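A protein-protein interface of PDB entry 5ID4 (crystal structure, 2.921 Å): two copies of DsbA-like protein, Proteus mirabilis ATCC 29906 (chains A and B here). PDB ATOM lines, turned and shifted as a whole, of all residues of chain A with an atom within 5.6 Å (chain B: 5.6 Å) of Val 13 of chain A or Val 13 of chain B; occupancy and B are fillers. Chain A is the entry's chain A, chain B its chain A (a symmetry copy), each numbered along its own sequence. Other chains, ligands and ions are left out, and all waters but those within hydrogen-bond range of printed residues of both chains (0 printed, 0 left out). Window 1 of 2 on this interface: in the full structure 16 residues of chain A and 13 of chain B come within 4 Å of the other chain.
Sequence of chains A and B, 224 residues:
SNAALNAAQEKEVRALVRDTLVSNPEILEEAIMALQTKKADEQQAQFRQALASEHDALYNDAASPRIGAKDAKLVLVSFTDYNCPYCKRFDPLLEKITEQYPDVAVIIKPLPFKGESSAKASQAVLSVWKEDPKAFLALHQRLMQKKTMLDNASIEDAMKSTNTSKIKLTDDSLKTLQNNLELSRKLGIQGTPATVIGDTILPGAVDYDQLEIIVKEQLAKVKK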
ATOM      1  N   LEU A   5       0.472 -29.048  -2.397  1.00  0.00           N
ATOM      2  CA  LEU A   5      -0.329 -27.865  -2.107  1.00  0.00           C
ATOM      3  C   LEU A   5      -1.251 -27.624  -3.267  1.00  0.00           C
ATOM      4  O   LEU A   5      -0.929 -27.967  -4.402  1.00  0.00           O
ATOM      5  CB  LEU A   5       0.531 -26.633  -1.883  1.00  0.00           C
ATOM      6  CG  LEU A   5       1.435 -26.703  -0.663  1.00  0.00           C
ATOM      7  CD1 LEU A   5       2.827 -26.528  -1.141  1.00  0.00           C
ATOM      8  CD2 LEU A   5       1.080 -25.647   0.361  1.00  0.00           C
ATOM      9  N   ALA A   8      -3.917 -22.628  -5.609  1.00  0.00           N
ATOM     10  CA  ALA A   8      -4.030 -21.371  -4.868  1.00  0.00           C
ATOM     11  C   ALA A   8      -2.923 -21.210  -3.833  1.00  0.00           C
ATOM     12  O   ALA A   8      -2.141 -20.250  -3.889  1.00  0.00           O
ATOM     13  CB  ALA A   8      -5.358 -21.282  -4.191  1.00  0.00           C
ATOM     14  N   GLN A   9      -2.872 -22.146  -2.892  1.00  0.00           N
ATOM     15  CA  GLN A   9      -1.856 -22.150  -1.851  1.00  0.00           C
ATOM     16  C   GLN A   9      -0.446 -21.884  -2.391  1.00  0.00           C
ATOM     17  O   GLN A   9       0.242 -20.973  -1.936  1.00  0.00           O
ATOM     18  CB  GLN A   9      -1.876 -23.486  -1.114  1.00  0.00           C
ATOM     19  CG  GLN A   9      -3.013 -23.604  -0.124  1.00  0.00           C
ATOM     20  CD  GLN A   9      -3.211 -25.017   0.399  1.00  0.00           C
ATOM     21  OE1 GLN A   9      -2.905 -26.006  -0.278  1.00  0.00           O
ATOM     22  NE2 GLN A   9      -3.731 -25.118   1.620  1.00  0.00           N
ATOM     23  N   GLU A  10      -0.039 -22.686  -3.364  1.00  0.00           N
ATOM     24  CA  GLU A  10       1.271 -22.574  -3.995  1.00  0.00           C
ATOM     25  C   GLU A  10       1.521 -21.160  -4.521  1.00  0.00           C
ATOM     26  O   GLU A  10       2.497 -20.486  -4.134  1.00  0.00           O
ATOM     27  CB  GLU A  10       1.339 -23.615  -5.102  1.00  0.00           C
ATOM     28  CG  GLU A  10       2.359 -23.411  -6.190  1.00  0.00           C
ATOM     29  CD  GLU A  10       2.433 -24.647  -7.092  1.00  0.00           C
ATOM     30  OE1 GLU A  10       1.868 -25.701  -6.673  1.00  0.00           O
ATOM     31  OE2 GLU A  10       3.043 -24.564  -8.199  1.00  0.00           O
ATOM     32  N   LYS A  11       0.613 -20.701  -5.377  1.00  0.00           N
ATOM     33  CA  LYS A  11       0.662 -19.325  -5.849  1.00  0.00           C
ATOM     34  C   LYS A  11       0.850 -18.327  -4.699  1.00  0.00           C
ATOM     35  O   LYS A  11       1.714 -17.442  -4.763  1.00  0.00           O
ATOM     36  CB  LYS A  11      -0.615 -19.016  -6.617  1.00  0.00           C
ATOM     37  CG  LYS A  11      -0.920 -17.551  -6.838  1.00  0.00           C
ATOM     38  CD  LYS A  11      -2.169 -17.440  -7.707  1.00  0.00           C
ATOM     39  CE  LYS A  11      -2.586 -15.999  -7.995  1.00  0.00           C
ATOM     40  NZ  LYS A  11      -4.018 -15.947  -8.501  1.00  0.00           N
ATOM     41  N   GLU A  12       0.075 -18.481  -3.631  1.00  0.00           N
ATOM     42  CA  GLU A  12       0.233 -17.589  -2.491  1.00  0.00           C
ATOM     43  C   GLU A  12       1.630 -17.722  -1.903  1.00  0.00           C
ATOM     44  O   GLU A  12       2.256 -16.708  -1.581  1.00  0.00           O
ATOM     45  CB  GLU A  12      -0.804 -17.844  -1.391  1.00  0.00           C
ATOM     46  CG  GLU A  12      -0.878 -16.674  -0.386  1.00  0.00           C
ATOM     47  CD  GLU A  12      -1.806 -16.913   0.808  1.00  0.00           C
ATOM     48  OE1 GLU A  12      -1.394 -16.575   1.947  1.00  0.00           O
ATOM     49  OE2 GLU A  12      -2.931 -17.450   0.631  1.00  0.00           O
ATOM     50  N   VAL A  13       2.138 -18.946  -1.771  1.00  0.00           N
ATOM     51  CA  VAL A  13       3.520 -19.126  -1.309  1.00  0.00           C
ATOM     52  C   VAL A  13       4.493 -18.274  -2.149  1.00  0.00           C
ATOM     53  O   VAL A  13       5.271 -17.458  -1.609  1.00  0.00           O
ATOM     54  CB  VAL A  13       3.950 -20.606  -1.358  1.00  0.00           C
ATOM     55  CG1 VAL A  13       5.407 -20.762  -0.925  1.00  0.00           C
ATOM     56  CG2 VAL A  13       3.051 -21.415  -0.469  1.00  0.00           C
ATOM     57  N   ARG A  14       4.424 -18.458  -3.466  1.00  0.00           N
ATOM     58  CA  ARG A  14       5.262 -17.677  -4.354  1.00  0.00           C
ATOM     59  C   ARG A  14       5.136 -16.218  -4.015  1.00  0.00           C
ATOM     60  O   ARG A  14       6.145 -15.543  -3.797  1.00  0.00           O
ATOM     61  CB  ARG A  14       4.892 -17.906  -5.803  1.00  0.00           C
ATOM     62  CG  ARG A  14       5.422 -19.205  -6.306  1.00  0.00           C
ATOM     63  CD  ARG A  14       4.968 -19.490  -7.712  1.00  0.00           C
ATOM     64  NE  ARG A  14       5.028 -20.929  -7.978  1.00  0.00           N
ATOM     65  CZ  ARG A  14       6.086 -21.562  -8.488  1.00  0.00           C
ATOM     66  NH1 ARG A  14       7.200 -20.877  -8.814  1.00  0.00           N
ATOM     67  NH2 ARG A  14       6.020 -22.885  -8.676  1.00  0.00           N
ATOM     68  N   ALA A  15       3.900 -15.738  -3.932  1.00  0.00           N
ATOM     69  CA  ALA A  15       3.693 -14.324  -3.618  1.00  0.00           C
ATOM     70  C   ALA A  15       4.304 -13.972  -2.264  1.00  0.00           C
ATOM     71  O   ALA A  15       4.819 -12.865  -2.052  1.00  0.00           O
ATOM     72  CB  ALA A  15       2.222 -13.991  -3.638  1.00  0.00           C
ATOM     73  N   LEU A  16       4.263 -14.933  -1.355  1.00  0.00           N
ATOM     74  CA  LEU A  16       4.761 -14.705  -0.012  1.00  0.00           C
ATOM     75  C   LEU A  16       6.276 -14.569   0.041  1.00  0.00           C
ATOM     76  O   LEU A  16       6.802 -13.834   0.873  1.00  0.00           O
ATOM     77  CB  LEU A  16       4.335 -15.834   0.910  1.00  0.00           C
ATOM     78  CG  LEU A  16       3.043 -15.622   1.682  1.00  0.00           C
ATOM     79  CD1 LEU A  16       2.766 -16.912   2.426  1.00  0.00           C
ATOM     80  CD2 LEU A  16       3.123 -14.437   2.657  1.00  0.00           C
ATOM     81  N   VAL A  17       6.969 -15.310  -0.814  1.00  0.00           N
ATOM     82  CA  VAL A  17       8.408 -15.142  -0.946  1.00  0.00           C
ATOM     83  C   VAL A  17       8.747 -13.660  -1.213  1.00  0.00           C
ATOM     84  O   VAL A  17       9.434 -12.960  -0.427  1.00  0.00           O
ATOM     85  CB  VAL A  17       8.955 -16.002  -2.094  1.00  0.00           C
ATOM     86  CG1 VAL A  17      10.428 -15.755  -2.293  1.00  0.00           C
ATOM     87  CG2 VAL A  17       8.745 -17.451  -1.822  1.00  0.00           C
ATOM     88  N   ARG A  18       8.247 -13.198  -2.350  1.00  0.00           N
ATOM     89  CA  ARG A  18       8.438 -11.838  -2.785  1.00  0.00           C
ATOM     90  C   ARG A  18       8.091 -10.899  -1.666  1.00  0.00           C
ATOM     91  O   ARG A  18       8.936 -10.144  -1.202  1.00  0.00           O
ATOM     92  CB  ARG A  18       7.584 -11.550  -4.012  1.00  0.00           C
ATOM     93  CG  ARG A  18       7.391 -10.090  -4.336  1.00  0.00           C
ATOM     94  CD  ARG A  18       6.682  -9.929  -5.685  1.00  0.00           C
ATOM     95  NE  ARG A  18       6.762  -8.550  -6.154  1.00  0.00           N
ATOM     96  CZ  ARG A  18       5.837  -7.611  -5.954  1.00  0.00           C
ATOM     97  NH1 ARG A  18       4.699  -7.887  -5.308  1.00  0.00           N
ATOM     98  NH2 ARG A  18       6.055  -6.375  -6.412  1.00  0.00           N
ATOM     99  N   LEU B   5      -4.361 -19.668   2.539  1.00  0.00           N
ATOM    100  CA  LEU B   5      -3.711 -20.385   3.630  1.00  0.00           C
ATOM    101  C   LEU B   5      -4.204 -19.815   4.928  1.00  0.00           C
ATOM    102  O   LEU B   5      -4.558 -18.639   5.000  1.00  0.00           O
ATOM    103  CB  LEU B   5      -2.199 -20.266   3.571  1.00  0.00           C
ATOM    104  CG  LEU B   5      -1.558 -20.910   2.351  1.00  0.00           C
ATOM    105  CD1 LEU B   5      -0.806 -19.848   1.642  1.00  0.00           C
ATOM    106  CD2 LEU B   5      -0.645 -22.054   2.734  1.00  0.00           C
ATOM    107  N   ALA B   8      -1.815 -19.366  10.552  1.00  0.00           N
ATOM    108  CA  ALA B   8      -0.667 -20.162  10.991  1.00  0.00           C
ATOM    109  C   ALA B   8       0.233 -20.565   9.828  1.00  0.00           C
ATOM    110  O   ALA B   8       1.421 -20.217   9.799  1.00  0.00           O
ATOM    111  CB  ALA B   8      -1.125 -21.387  11.709  1.00  0.00           C
ATOM    112  N   GLN B   9      -0.341 -21.301   8.882  1.00  0.00           N
ATOM    113  CA  GLN B   9       0.375 -21.739   7.695  1.00  0.00           C
ATOM    114  C   GLN B   9       1.201 -20.621   7.048  1.00  0.00           C
ATOM    115  O   GLN B   9       2.404 -20.764   6.841  1.00  0.00           O
ATOM    116  CB  GLN B   9      -0.610 -22.300   6.674  1.00  0.00           C
ATOM    117  CG  GLN B   9      -1.084 -23.697   7.008  1.00  0.00           C
ATOM    118  CD  GLN B   9      -2.267 -24.149   6.167  1.00  0.00           C
ATOM    119  OE1 GLN B   9      -3.080 -23.337   5.708  1.00  0.00           O
ATOM    120  NE2 GLN B   9      -2.370 -25.460   5.964  1.00  0.00           N
ATOM    121  N   GLU B  10       0.537 -19.516   6.741  1.00  0.00           N
ATOM    122  CA  GLU B  10       1.164 -18.353   6.123  1.00  0.00           C
ATOM    123  C   GLU B  10       2.374 -17.874   6.927  1.00  0.00           C
ATOM    124  O   GLU B  10       3.509 -17.806   6.414  1.00  0.00           O
ATOM    125  CB  GLU B  10       0.102 -17.272   5.993  1.00  0.00           C
ATOM    126  CG  GLU B  10       0.570 -15.851   5.832  1.00  0.00           C
ATOM    127  CD  GLU B  10      -0.613 -14.933   5.503  1.00  0.00           C
ATOM    128  OE1 GLU B  10      -1.699 -15.491   5.167  1.00  0.00           O
ATOM    129  OE2 GLU B  10      -0.457 -13.678   5.583  1.00  0.00           O
ATOM    130  N   LYS B  11       2.132 -17.582   8.202  1.00  0.00           N
ATOM    131  CA  LYS B  11       3.219 -17.242   9.108  1.00  0.00           C
ATOM    132  C   LYS B  11       4.382 -18.238   9.012  1.00  0.00           C
ATOM    133  O   LYS B  11       5.548 -17.839   8.887  1.00  0.00           O
ATOM    134  CB  LYS B  11       2.682 -17.188  10.531  1.00  0.00           C
ATOM    135  CG  LYS B  11       3.716 -17.244  11.634  1.00  0.00           C
ATOM    136  CD  LYS B  11       3.007 -17.073  12.975  1.00  0.00           C
ATOM    137  CE  LYS B  11       3.951 -17.120  14.174  1.00  0.00           C
ATOM    138  NZ  LYS B  11       3.173 -17.351  15.459  1.00  0.00           N
ATOM    139  N   GLU B  12       4.075 -19.530   9.031  1.00  0.00           N
ATOM    140  CA  GLU B  12       5.133 -20.524   8.903  1.00  0.00           C
ATOM    141  C   GLU B  12       5.842 -20.375   7.565  1.00  0.00           C
ATOM    142  O   GLU B  12       7.074 -20.437   7.516  1.00  0.00           O
ATOM    143  CB  GLU B  12       4.616 -21.960   9.044  1.00  0.00           C
ATOM    144  CG  GLU B  12       5.763 -22.963   9.293  1.00  0.00           C
ATOM    145  CD  GLU B  12       5.334 -24.433   9.322  1.00  0.00           C
ATOM    146  OE1 GLU B  12       6.053 -25.265   8.714  1.00  0.00           O
ATOM    147  OE2 GLU B  12       4.282 -24.767   9.926  1.00  0.00           O
ATOM    148  N   VAL B  13       5.095 -20.164   6.483  1.00  0.00           N
ATOM    149  CA  VAL B  13       5.732 -19.909   5.185  1.00  0.00           C
ATOM    150  C   VAL B  13       6.770 -18.774   5.298  1.00  0.00           C
ATOM    151  O   VAL B  13       7.955 -18.943   4.939  1.00  0.00           O
ATOM    152  CB  VAL B  13       4.694 -19.557   4.099  1.00  0.00           C
ATOM    153  CG1 VAL B  13       5.382 -19.243   2.772  1.00  0.00           C
ATOM    154  CG2 VAL B  13       3.739 -20.703   3.934  1.00  0.00           C
ATOM    155  N   ARG B  14       6.317 -17.635   5.818  1.00  0.00           N
ATOM    156  CA  ARG B  14       7.218 -16.516   6.012  1.00  0.00           C
ATOM    157  C   ARG B  14       8.448 -16.978   6.740  1.00  0.00           C
ATOM    158  O   ARG B  14       9.568 -16.745   6.276  1.00  0.00           O
ATOM    159  CB  ARG B  14       6.550 -15.399   6.782  1.00  0.00           C
ATOM    160  CG  ARG B  14       5.624 -14.613   5.918  1.00  0.00           C
ATOM    161  CD  ARG B  14       4.875 -13.569   6.700  1.00  0.00           C
ATOM    162  NE  ARG B  14       3.642 -13.202   5.999  1.00  0.00           N
ATOM    163  CZ  ARG B  14       3.540 -12.211   5.112  1.00  0.00           C
ATOM    164  NH1 ARG B  14       4.613 -11.451   4.811  1.00  0.00           N
ATOM    165  NH2 ARG B  14       2.358 -11.982   4.531  1.00  0.00           N
ATOM    166  N   ALA B  15       8.247 -17.667   7.859  1.00  0.00           N
ATOM    167  CA  ALA B  15       9.395 -18.142   8.633  1.00  0.00           C
ATOM    168  C   ALA B  15      10.269 -19.072   7.794  1.00  0.00           C
ATOM    169  O   ALA B  15      11.501 -19.096   7.924  1.00  0.00           O
ATOM    170  CB  ALA B  15       8.930 -18.839   9.887  1.00  0.00           C
ATOM    171  N   LEU B  16       9.621 -19.821   6.916  1.00  0.00           N
ATOM    172  CA  LEU B  16      10.333 -20.786   6.098  1.00  0.00           C
ATOM    173  C   LEU B  16      11.220 -20.131   5.050  1.00  0.00           C
ATOM    174  O   LEU B  16      12.269 -20.669   4.704  1.00  0.00           O
ATOM    175  CB  LEU B  16       9.353 -21.716   5.403  1.00  0.00           C
ATOM    176  CG  LEU B  16       9.035 -23.017   6.121  1.00  0.00           C
ATOM    177  CD1 LEU B  16       7.960 -23.709   5.309  1.00  0.00           C
ATOM    178  CD2 LEU B  16      10.266 -23.923   6.280  1.00  0.00           C
ATOM    179  N   VAL B  17      10.775 -19.000   4.517  1.00  0.00           N
ATOM    180  CA  VAL B  17      11.614 -18.220   3.621  1.00  0.00           C
ATOM    181  C   VAL B  17      12.977 -17.932   4.286  1.00  0.00           C
ATOM    182  O   VAL B  17      14.068 -18.352   3.824  1.00  0.00           O
ATOM    183  CB  VAL B  17      10.937 -16.890   3.258  1.00  0.00           C
ATOM    184  CG1 VAL B  17      11.846 -16.041   2.408  1.00  0.00           C
ATOM    185  CG2 VAL B  17       9.668 -17.124   2.516  1.00  0.00           C
ATOM    186  N   ARG B  18      12.886 -17.199   5.386  1.00  0.00           N
ATOM    187  CA  ARG B  18      14.039 -16.826   6.165  1.00  0.00           C
ATOM    188  C   ARG B  18      14.877 -18.041   6.439  1.00  0.00           C
ATOM    189  O   ARG B  18      16.030 -18.106   6.032  1.00  0.00           O
ATOM    190  CB  ARG B  18      13.606 -16.168   7.469  1.00  0.00           C
ATOM    191  CG  ARG B  18      14.671 -16.079   8.532  1.00  0.00           C
ATOM    192  CD  ARG B  18      14.181 -15.238   9.714  1.00  0.00           C
ATOM    193  NE  ARG B  18      15.287 -14.886  10.599  1.00  0.00           N
ATOM    194  CZ  ARG B  18      15.650 -15.564  11.687  1.00  0.00           C
ATOM    195  NH1 ARG B  18      14.974 -16.647  12.086  1.00  0.00           N
ATOM    196  NH2 ARG B  18      16.707 -15.147  12.390  1.00  0.00           N
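The side-chain carboxylate (OE2) of Glu 12 of chain A is in hydrogen-bond range of the backbone NH (N) of Leu 5 of chain B (3.3 Å).
The side-chain carboxylate (OE1) of Glu 10 of chain B lies close to the side-chain carboxylate (OE1) of Glu 12 of chain A, at 3.4 Å.
The side-chain carboxylate (OE2) of Glu 10 of chain B is in salt-bridge range of the guanidinium group (NH2) of Arg 14 of chain B (3.5 Å).
Leu 5 of chain B touches Gln 9 of chain A (CD1 to O, 3.9 Å).
Val 13 of chain A touches Val 13 of chain B (CG1 to CG1, 3.997 Å).
Leu 16 of chain A touches Val 13 of chain B.
Arg 14 of chain B touches Leu 16 of chain A (NH2 to CD2, 3.2 Å).
Of the printed residues of chain B, Val 13 of chain A touches Val 13 (3.997 Å).
Of the printed residues of chain A, Val 13 of chain B touches Val 13 (3.997 Å) and Leu 16 (3.5 Å).
Of the printed residues of chain A, Leu 5 of chain B touches Gln 9 (3.9 Å) and Glu 12 (3.2 Å).
Of the printed residues of chain B, Leu 16 of chain A touches Val 13 (3.5 Å) and Arg 14 (3.2 Å).
Of the printed residues of chain A, Glu 10 of chain B touches Glu 12 (3.4 Å).
Of the printed residues of chain A, Arg 14 of chain B touches Leu 16 (3.2 Å).
Of the printed residues of chain B, Gln 9 of chain A touches Leu 5 (3.9 Å).
The nearest printed residue of chain A that does not touch Leu 5 of chain B is Val 13 of chain A (4.6 Å).
Of the 12 printed residues of chain A, 4 touch a printed residue of chain B.
Hydrophobic or aromatic side chains of chain A that line the printed part of chain B: Val 13 and Leu 16.
Printed residues of chain B that touch a printed residue of chain A: Leu 5, Glu 10, Val 13 and Arg 14.
Among the printed residues, no Asp or Glu carboxylate lies within 4 Å of a Lys or Arg side-chain nitrogen of the other chain.
Gln 9 of chain A touches Leu 5 of chain B, but with the chains exchanged Leu 5 of chain A does not touch Gln 9 of chain B (6.6 Å).
Glu 12 of chain A touches Leu 5 of chain B, but with the chains exchanged Leu 5 of chain A does not touch Glu 12 of chain B (9.7 Å).
Leu 16 of chain A touches Val 13 of chain B, but with the chains exchanged Val 13 of chain A does not touch Leu 16 of chain B (7.4 Å).
Leu 16 of chain A touches Arg 14 of chain B, but with the chains exchanged Arg 14 of chain A does not touch Leu 16 of chain B (10.7 Å).
Of the 6 pairs that touch across the chains among the printed residues, 1 has its exchanged pair printed and touching as well.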
